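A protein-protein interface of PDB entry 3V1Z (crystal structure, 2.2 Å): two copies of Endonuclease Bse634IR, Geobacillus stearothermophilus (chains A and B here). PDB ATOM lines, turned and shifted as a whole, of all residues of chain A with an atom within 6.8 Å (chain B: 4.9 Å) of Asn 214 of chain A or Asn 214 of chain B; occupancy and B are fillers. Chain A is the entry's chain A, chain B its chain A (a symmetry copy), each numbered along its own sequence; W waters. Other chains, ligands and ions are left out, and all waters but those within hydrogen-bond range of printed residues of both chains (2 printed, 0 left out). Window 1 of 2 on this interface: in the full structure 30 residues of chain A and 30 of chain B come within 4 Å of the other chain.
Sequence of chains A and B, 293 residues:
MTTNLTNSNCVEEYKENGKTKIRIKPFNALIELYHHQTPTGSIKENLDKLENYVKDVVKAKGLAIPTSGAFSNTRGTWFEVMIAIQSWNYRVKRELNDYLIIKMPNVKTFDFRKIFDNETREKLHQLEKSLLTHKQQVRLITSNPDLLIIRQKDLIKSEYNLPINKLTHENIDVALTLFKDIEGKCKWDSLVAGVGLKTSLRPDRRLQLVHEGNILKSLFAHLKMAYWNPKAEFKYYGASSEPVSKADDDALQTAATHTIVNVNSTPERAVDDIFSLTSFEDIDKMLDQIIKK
Of the printed residues of chain B, His 211 of chain A touches Val 210 (3.4 Å).
Of chain B, only Asn 214 (3.5 Å) and Thr 257 (2.8 Å) come within 4 Å of Asn 214 of chain A.
Leu 219 of chain A touches none of the printed residues of chain B.
Ala 255 of chain A touches none of the printed residues of chain B.
Of the printed residues of chain A, His 211 of chain B touches Val 210 (3.4 Å).
Of the printed residues of chain A, Asn 214 of chain B touches Asn 214 and Thr 257.
Val 210 of chain A touches His 211 of chain B (CG1 to CE1, 3.4 Å).
His 211 of chain A touches Val 210 of chain B.
CD1 of Ile 215 of chain A touches CG2 of Thr 257 of chain B (3.6 Å).
OG of Ser 218 of chain A touches CG2 of Thr 257 of chain B, 3.7 Å away.
CD1 of Ile 215 of chain B touches CG2 of Thr 257 of chain A (3.6 Å).
Thr 257 of chain A touches Ser 218 of chain B.
CA of His 258 of chain A touches CA of His 258 of chain B, at 3.9 Å.
Val 210 of chain A touches His 211 of chain B, and with the chains exchanged His 211 of chain A touches Val 210 of chain B.
Ile 215 of chain A touches Thr 257 of chain B, and with the chains exchanged Thr 257 of chain A touches Ile 215 of chain B.
Ser 218 of chain A touches Thr 257 of chain B, and with the chains exchanged Thr 257 of chain A touches Ser 218 of chain B.
His 258 of chain B touches its own counterpart, His 258 of chain A.
Water W1 lies within hydrogen-bond range of the side-chain hydroxyl of Ser 218 of chain A (2.8 Å) and the backbone carbonyl oxygen of Thr 257 of chain B (2.9 Å).
Water W2 bridges the side-chain hydroxyl (OG) of Ser 218 of chain B (2.8 Å) and the backbone carbonyl oxygen (O) of Thr 257 of chain A (2.9 Å).
The backbone NH (N) of Thr 257 of chain A lies within hydrogen-bond range of the side-chain amide oxygen (OD1) of Asn 214 of chain A, 3.1 Å away.
OD1 of Asn 214 of chain B sits at hydrogen-bond distance from N of Thr 257 of chain B.
Printed residues of chain A that touch a printed residue of chain B: Val 210, His 211, Asn 214, Ile 215, Ser 218, Thr 257 and His 258.
Hydrophobic or aromatic side chains of chain A within 4 Å of the printed part of chain B: Val 210, His 211, Ile 215 and His 258.
Along chain A the printed residues that touch a printed residue of chain B span positions 210 to 258.
Of the 14 printed residues of chain B, 7 touch a printed residue of chain A.
Among the printed residues, no Asp or Glu carboxylate lies within 4 Å of a Lys or Arg side-chain nitrogen of the other chain.
The side-chain hydroxyl (OG1) of Thr 257 of chain B is in hydrogen-bond range of a ring nitrogen (ND1) of His 258 of chain A (3.4 Å).
The side-chain hydroxyl of Thr 257 of chain A sits at hydrogen-bond distance from the side-chain amide nitrogen of Asn 214 of chain B, at 2.8 Å.
The side-chain amide nitrogen (ND2) of Asn 214 of chain A sits at hydrogen-bond distance from the side-chain hydroxyl (OG1) of Thr 257 of chain B (2.8 Å).
The side-chain amide nitrogen (ND2) of Asn 214 of chain A lies close to the side-chain amide nitrogen (ND2) of Asn 214 of chain B (3.5 Å).
ND1 of His 258 of chain B lies within hydrogen-bond range of OG1 of Thr 257 of chain A.
The side-chain hydroxyl (OG1) of Thr 257 of chain A lies within hydrogen-bond range of the side-chain hydroxyl (OG1) of Thr 257 of chain B (3.3 Å).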
ATOM      1  N   LEU A 140     -37.558  23.836 -15.940  1.00  0.00           N
ATOM      2  CA  LEU A 140     -36.336  24.611 -15.738  1.00  0.00           C
ATOM      3  C   LEU A 140     -36.703  25.914 -15.040  1.00  0.00           C
ATOM      4  O   LEU A 140     -36.885  26.952 -15.682  1.00  0.00           O
ATOM      5  CB  LEU A 140     -35.637  24.884 -17.075  1.00  0.00           C
ATOM      6  CG  LEU A 140     -35.013  23.695 -17.814  1.00  0.00           C
ATOM      7  CD1 LEU A 140     -34.743  24.059 -19.261  1.00  0.00           C
ATOM      8  CD2 LEU A 140     -33.731  23.203 -17.123  1.00  0.00           C
ATOM      9  N   LEU A 209     -26.814  30.978  -6.290  1.00  0.00           N
ATOM     10  CA  LEU A 209     -26.165  31.631  -7.434  1.00  0.00           C
ATOM     11  C   LEU A 209     -25.708  30.592  -8.460  1.00  0.00           C
ATOM     12  O   LEU A 209     -25.744  30.849  -9.660  1.00  0.00           O
ATOM     13  CB  LEU A 209     -24.977  32.492  -6.982  1.00  0.00           C
ATOM     14  CG  LEU A 209     -25.233  33.679  -6.041  1.00  0.00           C
ATOM     15  CD1 LEU A 209     -23.924  34.254  -5.521  1.00  0.00           C
ATOM     16  CD2 LEU A 209     -26.065  34.778  -6.715  1.00  0.00           C
ATOM     17  N   VAL A 210     -25.285  29.423  -7.978  1.00  0.00           N
ATOM     18  CA  VAL A 210     -24.918  28.312  -8.851  1.00  0.00           C
ATOM     19  C   VAL A 210     -26.152  27.758  -9.569  1.00  0.00           C
ATOM     20  O   VAL A 210     -26.115  27.549 -10.770  1.00  0.00           O
ATOM     21  CB  VAL A 210     -24.186  27.180  -8.089  1.00  0.00           C
ATOM     22  CG1 VAL A 210     -23.808  26.061  -9.044  1.00  0.00           C
ATOM     23  CG2 VAL A 210     -22.942  27.715  -7.383  1.00  0.00           C
ATOM     24  N   HIS A 211     -27.243  27.533  -8.841  1.00  0.00           N
ATOM     25  CA  HIS A 211     -28.481  27.073  -9.470  1.00  0.00           C
ATOM     26  C   HIS A 211     -28.895  28.032 -10.584  1.00  0.00           C
ATOM     27  O   HIS A 211     -29.145  27.611 -11.710  1.00  0.00           O
ATOM     28  CB  HIS A 211     -29.620  26.909  -8.452  1.00  0.00           C
ATOM     29  CG  HIS A 211     -30.943  26.604  -9.085  1.00  0.00           C
ATOM     30  ND1 HIS A 211     -31.290  25.340  -9.509  1.00  0.00           N
ATOM     31  CD2 HIS A 211     -31.992  27.404  -9.393  1.00  0.00           C
ATOM     32  CE1 HIS A 211     -32.501  25.372 -10.039  1.00  0.00           C
ATOM     33  NE2 HIS A 211     -32.949  26.613  -9.982  1.00  0.00           N
ATOM     34  N   GLU A 212     -28.948  29.316 -10.251  1.00  0.00           N
ATOM     35  CA  GLU A 212     -29.311  30.372 -11.195  1.00  0.00           C
ATOM     36  C   GLU A 212     -28.473  30.349 -12.471  1.00  0.00           C
ATOM     37  O   GLU A 212     -29.021  30.352 -13.571  1.00  0.00           O
ATOM     38  CB  GLU A 212     -29.183  31.733 -10.524  1.00  0.00           C
ATOM     39  CG  GLU A 212     -29.610  32.888 -11.403  1.00  0.00           C
ATOM     40  CD  GLU A 212     -31.094  33.125 -11.370  1.00  0.00           C
ATOM     41  OE1 GLU A 212     -31.573  33.785 -10.420  1.00  0.00           O
ATOM     42  OE2 GLU A 212     -31.780  32.659 -12.303  1.00  0.00           O
ATOM     43  N   GLY A 213     -27.148  30.322 -12.311  1.00  0.00           N
ATOM     44  CA  GLY A 213     -26.238  30.272 -13.444  1.00  0.00           C
ATOM     45  C   GLY A 213     -26.436  29.007 -14.253  1.00  0.00           C
ATOM     46  O   GLY A 213     -26.553  29.055 -15.485  1.00  0.00           O
ATOM     47  N   ASN A 214     -26.487  27.875 -13.554  1.00  0.00           N
ATOM     48  CA  ASN A 214     -26.707  26.579 -14.187  1.00  0.00           C
ATOM     49  C   ASN A 214     -27.963  26.541 -15.064  1.00  0.00           C
ATOM     50  O   ASN A 214     -27.903  26.097 -16.214  1.00  0.00           O
ATOM     51  CB  ASN A 214     -26.747  25.460 -13.139  1.00  0.00           C
ATOM     52  CG  ASN A 214     -26.652  24.082 -13.758  1.00  0.00           C
ATOM     53  OD1 ASN A 214     -25.649  23.741 -14.375  1.00  0.00           O
ATOM     54  ND2 ASN A 214     -27.701  23.283 -13.604  1.00  0.00           N
ATOM     55  N   ILE A 215     -29.085  27.017 -14.532  1.00  0.00           N
ATOM     56  CA  ILE A 215     -30.356  26.982 -15.264  1.00  0.00           C
ATOM     57  C   ILE A 215     -30.360  27.948 -16.445  1.00  0.00           C
ATOM     58  O   ILE A 215     -30.906  27.623 -17.506  1.00  0.00           O
ATOM     59  CB  ILE A 215     -31.592  27.238 -14.336  1.00  0.00           C
ATOM     60  CG1 ILE A 215     -31.687  26.175 -13.235  1.00  0.00           C
ATOM     61  CG2 ILE A 215     -32.913  27.301 -15.127  1.00  0.00           C
ATOM     62  CD1 ILE A 215     -31.612  24.728 -13.706  1.00  0.00           C
ATOM     63  N   LEU A 216     -29.757  29.123 -16.254  1.00  0.00           N
ATOM     64  CA  LEU A 216     -29.750  30.172 -17.266  1.00  0.00           C
ATOM     65  C   LEU A 216     -28.878  29.790 -18.453  1.00  0.00           C
ATOM     66  O   LEU A 216     -29.246  30.041 -19.603  1.00  0.00           O
ATOM     67  CB  LEU A 216     -29.281  31.511 -16.677  1.00  0.00           C
ATOM     68  CG  LEU A 216     -30.211  32.305 -15.749  1.00  0.00           C
ATOM     69  CD1 LEU A 216     -29.467  33.493 -15.146  1.00  0.00           C
ATOM     70  CD2 LEU A 216     -31.468  32.773 -16.467  1.00  0.00           C
ATOM     71  N   LYS A 217     -27.729  29.186 -18.153  1.00  0.00           N
ATOM     72  CA  LYS A 217     -26.790  28.705 -19.154  1.00  0.00           C
ATOM     73  C   LYS A 217     -27.306  27.473 -19.883  1.00  0.00           C
ATOM     74  O   LYS A 217     -26.880  27.194 -21.004  1.00  0.00           O
ATOM     75  CB  LYS A 217     -25.419  28.420 -18.517  1.00  0.00           C
ATOM     76  CG  LYS A 217     -24.701  29.679 -18.067  1.00  0.00           C
ATOM     77  CD  LYS A 217     -23.311  29.392 -17.540  1.00  0.00           C
ATOM     78  CE  LYS A 217     -22.566  30.699 -17.327  1.00  0.00           C
ATOM     79  NZ  LYS A 217     -21.135  30.455 -17.057  1.00  0.00           N
ATOM     80  N   SER A 218     -28.212  26.744 -19.233  1.00  0.00           N
ATOM     81  CA  SER A 218     -28.881  25.581 -19.813  1.00  0.00           C
ATOM     82  C   SER A 218     -29.975  26.016 -20.796  1.00  0.00           C
ATOM     83  O   SER A 218     -30.127  25.420 -21.869  1.00  0.00           O
ATOM     84  CB  SER A 218     -29.441  24.672 -18.702  1.00  0.00           C
ATOM     85  OG  SER A 218     -30.419  23.757 -19.190  1.00  0.00           O
ATOM     86  N   LEU A 219     -30.725  27.058 -20.436  1.00  0.00           N
ATOM     87  CA  LEU A 219     -31.675  27.668 -21.371  1.00  0.00           C
ATOM     88  C   LEU A 219     -30.947  28.314 -22.562  1.00  0.00           C
ATOM     89  O   LEU A 219     -31.425  28.251 -23.689  1.00  0.00           O
ATOM     90  CB  LEU A 219     -32.559  28.707 -20.669  1.00  0.00           C
ATOM     91  CG  LEU A 219     -33.622  28.233 -19.663  1.00  0.00           C
ATOM     92  CD1 LEU A 219     -34.044  29.382 -18.745  1.00  0.00           C
ATOM     93  CD2 LEU A 219     -34.833  27.640 -20.362  1.00  0.00           C
ATOM     94  N   TYR A 236     -22.655  34.417 -16.279  1.00  0.00           N
ATOM     95  CA  TYR A 236     -23.353  34.709 -15.044  1.00  0.00           C
ATOM     96  C   TYR A 236     -22.392  35.039 -13.917  1.00  0.00           C
ATOM     97  O   TYR A 236     -21.382  34.364 -13.715  1.00  0.00           O
ATOM     98  CB  TYR A 236     -24.280  33.560 -14.647  1.00  0.00           C
ATOM     99  CG  TYR A 236     -25.212  33.955 -13.534  1.00  0.00           C
ATOM    100  CD1 TYR A 236     -26.294  34.793 -13.785  1.00  0.00           C
ATOM    101  CD2 TYR A 236     -24.988  33.530 -12.223  1.00  0.00           C
ATOM    102  CE1 TYR A 236     -27.140  35.182 -12.778  1.00  0.00           C
ATOM    103  CE2 TYR A 236     -25.847  33.911 -11.199  1.00  0.00           C
ATOM    104  CZ  TYR A 236     -26.920  34.743 -11.494  1.00  0.00           C
ATOM    105  OH  TYR A 236     -27.785  35.140 -10.508  1.00  0.00           O
ATOM    106  N   ALA A 255     -19.405  23.798 -11.345  1.00  0.00           N
ATOM    107  CA  ALA A 255     -19.645  23.713 -12.778  1.00  0.00           C
ATOM    108  C   ALA A 255     -21.117  23.781 -13.121  1.00  0.00           C
ATOM    109  O   ALA A 255     -21.969  23.356 -12.341  1.00  0.00           O
ATOM    110  CB  ALA A 255     -19.053  22.424 -13.328  1.00  0.00           C
ATOM    111  N   ALA A 256     -21.404  24.335 -14.297  1.00  0.00           N
ATOM    112  CA  ALA A 256     -22.674  24.104 -14.967  1.00  0.00           C
ATOM    113  C   ALA A 256     -22.592  22.652 -15.446  1.00  0.00           C
ATOM    114  O   ALA A 256     -21.830  22.338 -16.361  1.00  0.00           O
ATOM    115  CB  ALA A 256     -22.836  25.065 -16.142  1.00  0.00           C
ATOM    116  N   THR A 257     -23.348  21.772 -14.799  1.00  0.00           N
ATOM    117  CA  THR A 257     -23.120  20.325 -14.890  1.00  0.00           C
ATOM    118  C   THR A 257     -23.263  19.709 -16.286  1.00  0.00           C
ATOM    119  O   THR A 257     -22.679  18.665 -16.561  1.00  0.00           O
ATOM    120  CB  THR A 257     -23.975  19.530 -13.865  1.00  0.00           C
ATOM    121  OG1 THR A 257     -25.356  19.872 -14.012  1.00  0.00           O
ATOM    122  CG2 THR A 257     -23.536  19.838 -12.449  1.00  0.00           C
ATOM    123  N   HIS A 258     -24.032  20.354 -17.161  1.00  0.00           N
ATOM    124  CA  HIS A 258     -24.195  19.874 -18.535  1.00  0.00           C
ATOM    125  C   HIS A 258     -22.916  19.993 -19.386  1.00  0.00           C
ATOM    126  O   HIS A 258     -22.824  19.415 -20.469  1.00  0.00           O
ATOM    127  CB  HIS A 258     -25.391  20.546 -19.222  1.00  0.00           C
ATOM    128  CG  HIS A 258     -25.391  22.041 -19.130  1.00  0.00           C
ATOM    129  ND1 HIS A 258     -25.721  22.718 -17.972  1.00  0.00           N
ATOM    130  CD2 HIS A 258     -25.120  22.990 -20.057  1.00  0.00           C
ATOM    131  CE1 HIS A 258     -25.645  24.018 -18.190  1.00  0.00           C
ATOM    132  NE2 HIS A 258     -25.285  24.210 -19.446  1.00  0.00           N
ATOM    133  N   THR A 259     -21.926  20.715 -18.872  1.00  0.00           N
ATOM    134  CA  THR A 259     -20.676  20.946 -19.587  1.00  0.00           C
ATOM    135  C   THR A 259     -19.565  19.978 -19.172  1.00  0.00           C
ATOM    136  O   THR A 259     -18.483  20.006 -19.749  1.00  0.00           O
ATOM    137  CB  THR A 259     -20.173  22.399 -19.397  1.00  0.00           C
ATOM    138  OG1 THR A 259     -19.783  22.603 -18.032  1.00  0.00           O
ATOM    139  CG2 THR A 259     -21.249  23.412 -19.782  1.00  0.00           C
ATOM    140  N   ARG A 269     -17.814  27.119 -15.554  1.00  0.00           N
ATOM    141  CA  ARG A 269     -18.391  27.517 -14.274  1.00  0.00           C
ATOM    142  C   ARG A 269     -19.824  27.990 -14.499  1.00  0.00           C
ATOM    143  O   ARG A 269     -20.096  28.681 -15.480  1.00  0.00           O
ATOM    144  CB  ARG A 269     -17.575  28.655 -13.659  1.00  0.00           C
ATOM    145  CG  ARG A 269     -16.236  28.225 -13.107  1.00  0.00           C
ATOM    146  CD  ARG A 269     -15.416  29.410 -12.642  1.00  0.00           C
ATOM    147  NE  ARG A 269     -16.076  30.162 -11.573  1.00  0.00           N
ATOM    148  CZ  ARG A 269     -15.488  31.110 -10.845  1.00  0.00           C
ATOM    149  NH1 ARG A 269     -14.209  31.424 -11.060  1.00  0.00           N
ATOM    150  NH2 ARG A 269     -16.180  31.740  -9.897  1.00  0.00           N
ATOM    151  N   ALA A 270     -20.734  27.613 -13.602  1.00  0.00           N
ATOM    152  CA  ALA A 270     -22.107  28.144 -13.622  1.00  0.00           C
ATOM    153  C   ALA A 270     -22.106  29.654 -13.311  1.00  0.00           C
ATOM    154  O   ALA A 270     -22.870  30.427 -13.899  1.00  0.00           O
ATOM    155  CB  ALA A 270     -22.990  27.390 -12.637  1.00  0.00           C
ATOM    156  N   VAL A 271     -21.233  30.053 -12.388  1.00  0.00           N
ATOM    157  CA  VAL A 271     -21.000  31.457 -12.060  1.00  0.00           C
ATOM    158  C   VAL A 271     -19.577  31.813 -12.446  1.00  0.00           C
ATOM    159  O   VAL A 271     -18.603  31.337 -11.835  1.00  0.00           O
ATOM    160  CB  VAL A 271     -21.226  31.763 -10.554  1.00  0.00           C
ATOM    161  CG1 VAL A 271     -20.996  33.246 -10.261  1.00  0.00           C
ATOM    162  CG2 VAL A 271     -22.626  31.336 -10.116  1.00  0.00           C
ATOM    163  N   VAL B 210     -32.664  21.636  -5.432  1.00  0.00           N
ATOM    164  CA  VAL B 210     -32.360  21.367  -6.835  1.00  0.00           C
ATOM    165  C   VAL B 210     -30.845  21.345  -7.064  1.00  0.00           C
ATOM    166  O   VAL B 210     -30.339  20.438  -7.703  1.00  0.00           O
ATOM    167  CB  VAL B 210     -33.033  22.381  -7.790  1.00  0.00           C
ATOM    168  CG1 VAL B 210     -32.703  22.044  -9.234  1.00  0.00           C
ATOM    169  CG2 VAL B 210     -34.546  22.399  -7.586  1.00  0.00           C
ATOM    170  N   HIS B 211     -30.125  22.332  -6.537  1.00  0.00           N
ATOM    171  CA  HIS B 211     -28.667  22.341  -6.653  1.00  0.00           C
ATOM    172  C   HIS B 211     -28.086  21.040  -6.103  1.00  0.00           C
ATOM    173  O   HIS B 211     -27.306  20.369  -6.773  1.00  0.00           O
ATOM    174  CB  HIS B 211     -28.038  23.550  -5.947  1.00  0.00           C
ATOM    175  CG  HIS B 211     -26.541  23.499  -5.900  1.00  0.00           C
ATOM    176  ND1 HIS B 211     -25.752  23.856  -6.972  1.00  0.00           N
ATOM    177  CD2 HIS B 211     -25.690  23.106  -4.923  1.00  0.00           C
ATOM    178  CE1 HIS B 211     -24.479  23.696  -6.652  1.00  0.00           C
ATOM    179  NE2 HIS B 211     -24.413  23.241  -5.414  1.00  0.00           N
ATOM    180  N   GLU B 212     -28.491  20.695  -4.885  1.00  0.00           N
ATOM    181  CA  GLU B 212     -28.048  19.476  -4.211  1.00  0.00           C
ATOM    182  C   GLU B 212     -28.263  18.218  -5.048  1.00  0.00           C
ATOM    183  O   GLU B 212     -27.334  17.434  -5.234  1.00  0.00           O
ATOM    184  CB  GLU B 212     -28.769  19.332  -2.877  1.00  0.00           C
ATOM    185  CG  GLU B 212     -28.321  18.134  -2.069  1.00  0.00           C
ATOM    186  CD  GLU B 212     -27.086  18.409  -1.257  1.00  0.00           C
ATOM    187  OE1 GLU B 212     -27.213  18.993  -0.157  1.00  0.00           O
ATOM    188  OE2 GLU B 212     -25.989  18.031  -1.716  1.00  0.00           O
ATOM    189  N   GLY B 213     -29.486  18.038  -5.549  1.00  0.00           N
ATOM    190  CA  GLY B 213     -29.815  16.893  -6.384  1.00  0.00           C
ATOM    191  C   GLY B 213     -29.001  16.893  -7.661  1.00  0.00           C
ATOM    192  O   GLY B 213     -28.410  15.871  -8.034  1.00  0.00           O
ATOM    193  N   ASN B 214     -28.961  18.048  -8.322  1.00  0.00           N
ATOM    194  CA  ASN B 214     -28.191  18.214  -9.550  1.00  0.00           C
ATOM    195  C   ASN B 214     -26.720  17.811  -9.400  1.00  0.00           C
ATOM    196  O   ASN B 214     -26.197  17.057 -10.225  1.00  0.00           O
ATOM    197  CB  ASN B 214     -28.306  19.651 -10.075  1.00  0.00           C
ATOM    198  CG  ASN B 214     -27.799  19.792 -11.494  1.00  0.00           C
ATOM    199  OD1 ASN B 214     -28.348  19.199 -12.416  1.00  0.00           O
ATOM    200  ND2 ASN B 214     -26.742  20.574 -11.677  1.00  0.00           N
ATOM    201  N   ILE B 215     -26.067  18.296  -8.348  1.00  0.00           N
ATOM    202  CA  ILE B 215     -24.642  18.016  -8.136  1.00  0.00           C
ATOM    203  C   ILE B 215     -24.397  16.555  -7.771  1.00  0.00           C
ATOM    204  O   ILE B 215     -23.406  15.965  -8.217  1.00  0.00           O
ATOM    205  CB  ILE B 215     -23.994  18.968  -7.074  1.00  0.00           C
ATOM    206  CG1 ILE B 215     -24.096  20.434  -7.509  1.00  0.00           C
ATOM    207  CG2 ILE B 215     -22.526  18.603  -6.780  1.00  0.00           C
ATOM    208  CD1 ILE B 215     -23.615  20.738  -8.922  1.00  0.00           C
ATOM    209  N   LEU B 216     -25.295  15.985  -6.965  1.00  0.00           N
ATOM    210  CA  LEU B 216     -25.149  14.621  -6.471  1.00  0.00           C
ATOM    211  C   LEU B 216     -25.340  13.606  -7.587  1.00  0.00           C
ATOM    212  O   LEU B 216     -24.611  12.613  -7.659  1.00  0.00           O
ATOM    213  CB  LEU B 216     -26.130  14.336  -5.325  1.00  0.00           C
ATOM    214  CG  LEU B 216     -25.884  14.946  -3.938  1.00  0.00           C
ATOM    215  CD1 LEU B 216     -27.076  14.678  -3.024  1.00  0.00           C
ATOM    216  CD2 LEU B 216     -24.601  14.426  -3.306  1.00  0.00           C
ATOM    217  N   LYS B 217     -26.324  13.871  -8.446  1.00  0.00           N
ATOM    218  CA  LYS B 217     -26.625  13.043  -9.603  1.00  0.00           C
ATOM    219  C   LYS B 217     -25.573  13.171 -10.693  1.00  0.00           C
ATOM    220  O   LYS B 217     -25.424  12.269 -11.518  1.00  0.00           O
ATOM    221  CB  LYS B 217     -28.021  13.377 -10.158  1.00  0.00           C
ATOM    222  CG  LYS B 217     -29.145  12.953  -9.231  1.00  0.00           C
ATOM    223  CD  LYS B 217     -30.512  13.192  -9.838  1.00  0.00           C
ATOM    224  CE  LYS B 217     -31.576  12.541  -8.970  1.00  0.00           C
ATOM    225  NZ  LYS B 217     -32.885  12.533  -9.654  1.00  0.00           N
ATOM    226  N   SER B 218     -24.859  14.296 -10.689  1.00  0.00           N
ATOM    227  CA  SER B 218     -23.749  14.551 -11.605  1.00  0.00           C
ATOM    228  C   SER B 218     -22.494  13.787 -11.165  1.00  0.00           C
ATOM    229  O   SER B 218     -21.777  13.224 -12.002  1.00  0.00           O
ATOM    230  CB  SER B 218     -23.483  16.065 -11.720  1.00  0.00           C
ATOM    231  OG  SER B 218     -22.199  16.351 -12.268  1.00  0.00           O
ATOM    232  N   ALA B 255     -35.086  20.159 -13.769  1.00  0.00           N
ATOM    233  CA  ALA B 255     -34.272  19.066 -14.279  1.00  0.00           C
ATOM    234  C   ALA B 255     -32.855  19.108 -13.754  1.00  0.00           C
ATOM    235  O   ALA B 255     -32.317  20.179 -13.470  1.00  0.00           O
ATOM    236  CB  ALA B 255     -34.253  19.099 -15.801  1.00  0.00           C
ATOM    237  N   ALA B 256     -32.262  17.925 -13.615  1.00  0.00           N
ATOM    238  CA  ALA B 256     -30.815  17.793 -13.543  1.00  0.00           C
ATOM    239  C   ALA B 256     -30.335  18.091 -14.966  1.00  0.00           C
ATOM    240  O   ALA B 256     -30.557  17.296 -15.879  1.00  0.00           O
ATOM    241  CB  ALA B 256     -30.432  16.378 -13.115  1.00  0.00           C
ATOM    242  N   THR B 257     -29.715  19.252 -15.150  1.00  0.00           N
ATOM    243  CA  THR B 257     -29.522  19.835 -16.483  1.00  0.00           C
ATOM    244  C   THR B 257     -28.678  19.010 -17.462  1.00  0.00           C
ATOM    245  O   THR B 257     -28.823  19.153 -18.673  1.00  0.00           O
ATOM    246  CB  THR B 257     -28.991  21.293 -16.416  1.00  0.00           C
ATOM    247  OG1 THR B 257     -27.800  21.341 -15.625  1.00  0.00           O
ATOM    248  CG2 THR B 257     -30.027  22.213 -15.808  1.00  0.00           C
ATOM    249  N   HIS B 258     -27.805  18.152 -16.939  1.00  0.00           N
ATOM    250  CA  HIS B 258     -26.985  17.283 -17.788  1.00  0.00           C
ATOM    251  C   HIS B 258     -27.796  16.200 -18.526  1.00  0.00           C
ATOM    252  O   HIS B 258     -27.294  15.560 -19.450  1.00  0.00           O
ATOM    253  CB  HIS B 258     -25.819  16.673 -16.999  1.00  0.00           C
ATOM    254  CG  HIS B 258     -26.225  16.011 -15.718  1.00  0.00           C
ATOM    255  ND1 HIS B 258     -26.571  16.723 -14.586  1.00  0.00           N
ATOM    256  CD2 HIS B 258     -26.322  14.703 -15.383  1.00  0.00           C
ATOM    257  CE1 HIS B 258     -26.870  15.881 -13.614  1.00  0.00           C
ATOM    258  NE2 HIS B 258     -26.725  14.649 -14.070  1.00  0.00           N
ATOM    259  N   ALA B 270     -33.940  16.720 -10.894  1.00  0.00           N
ATOM    260  CA  ALA B 270     -32.854  16.779  -9.901  1.00  0.00           C
ATOM    261  C   ALA B 270     -33.354  16.292  -8.527  1.00  0.00           C
ATOM    262  O   ALA B 270     -32.633  15.608  -7.792  1.00  0.00           O
ATOM    263  CB  ALA B 270     -32.292  18.190  -9.802  1.00  0.00           C
HETATM  264  O   HOH W   1     -28.899  21.574 -20.211  1.00  0.00           O
HETATM  265  O   HOH W   2     -22.584  16.204 -15.087  1.00  0.00           O
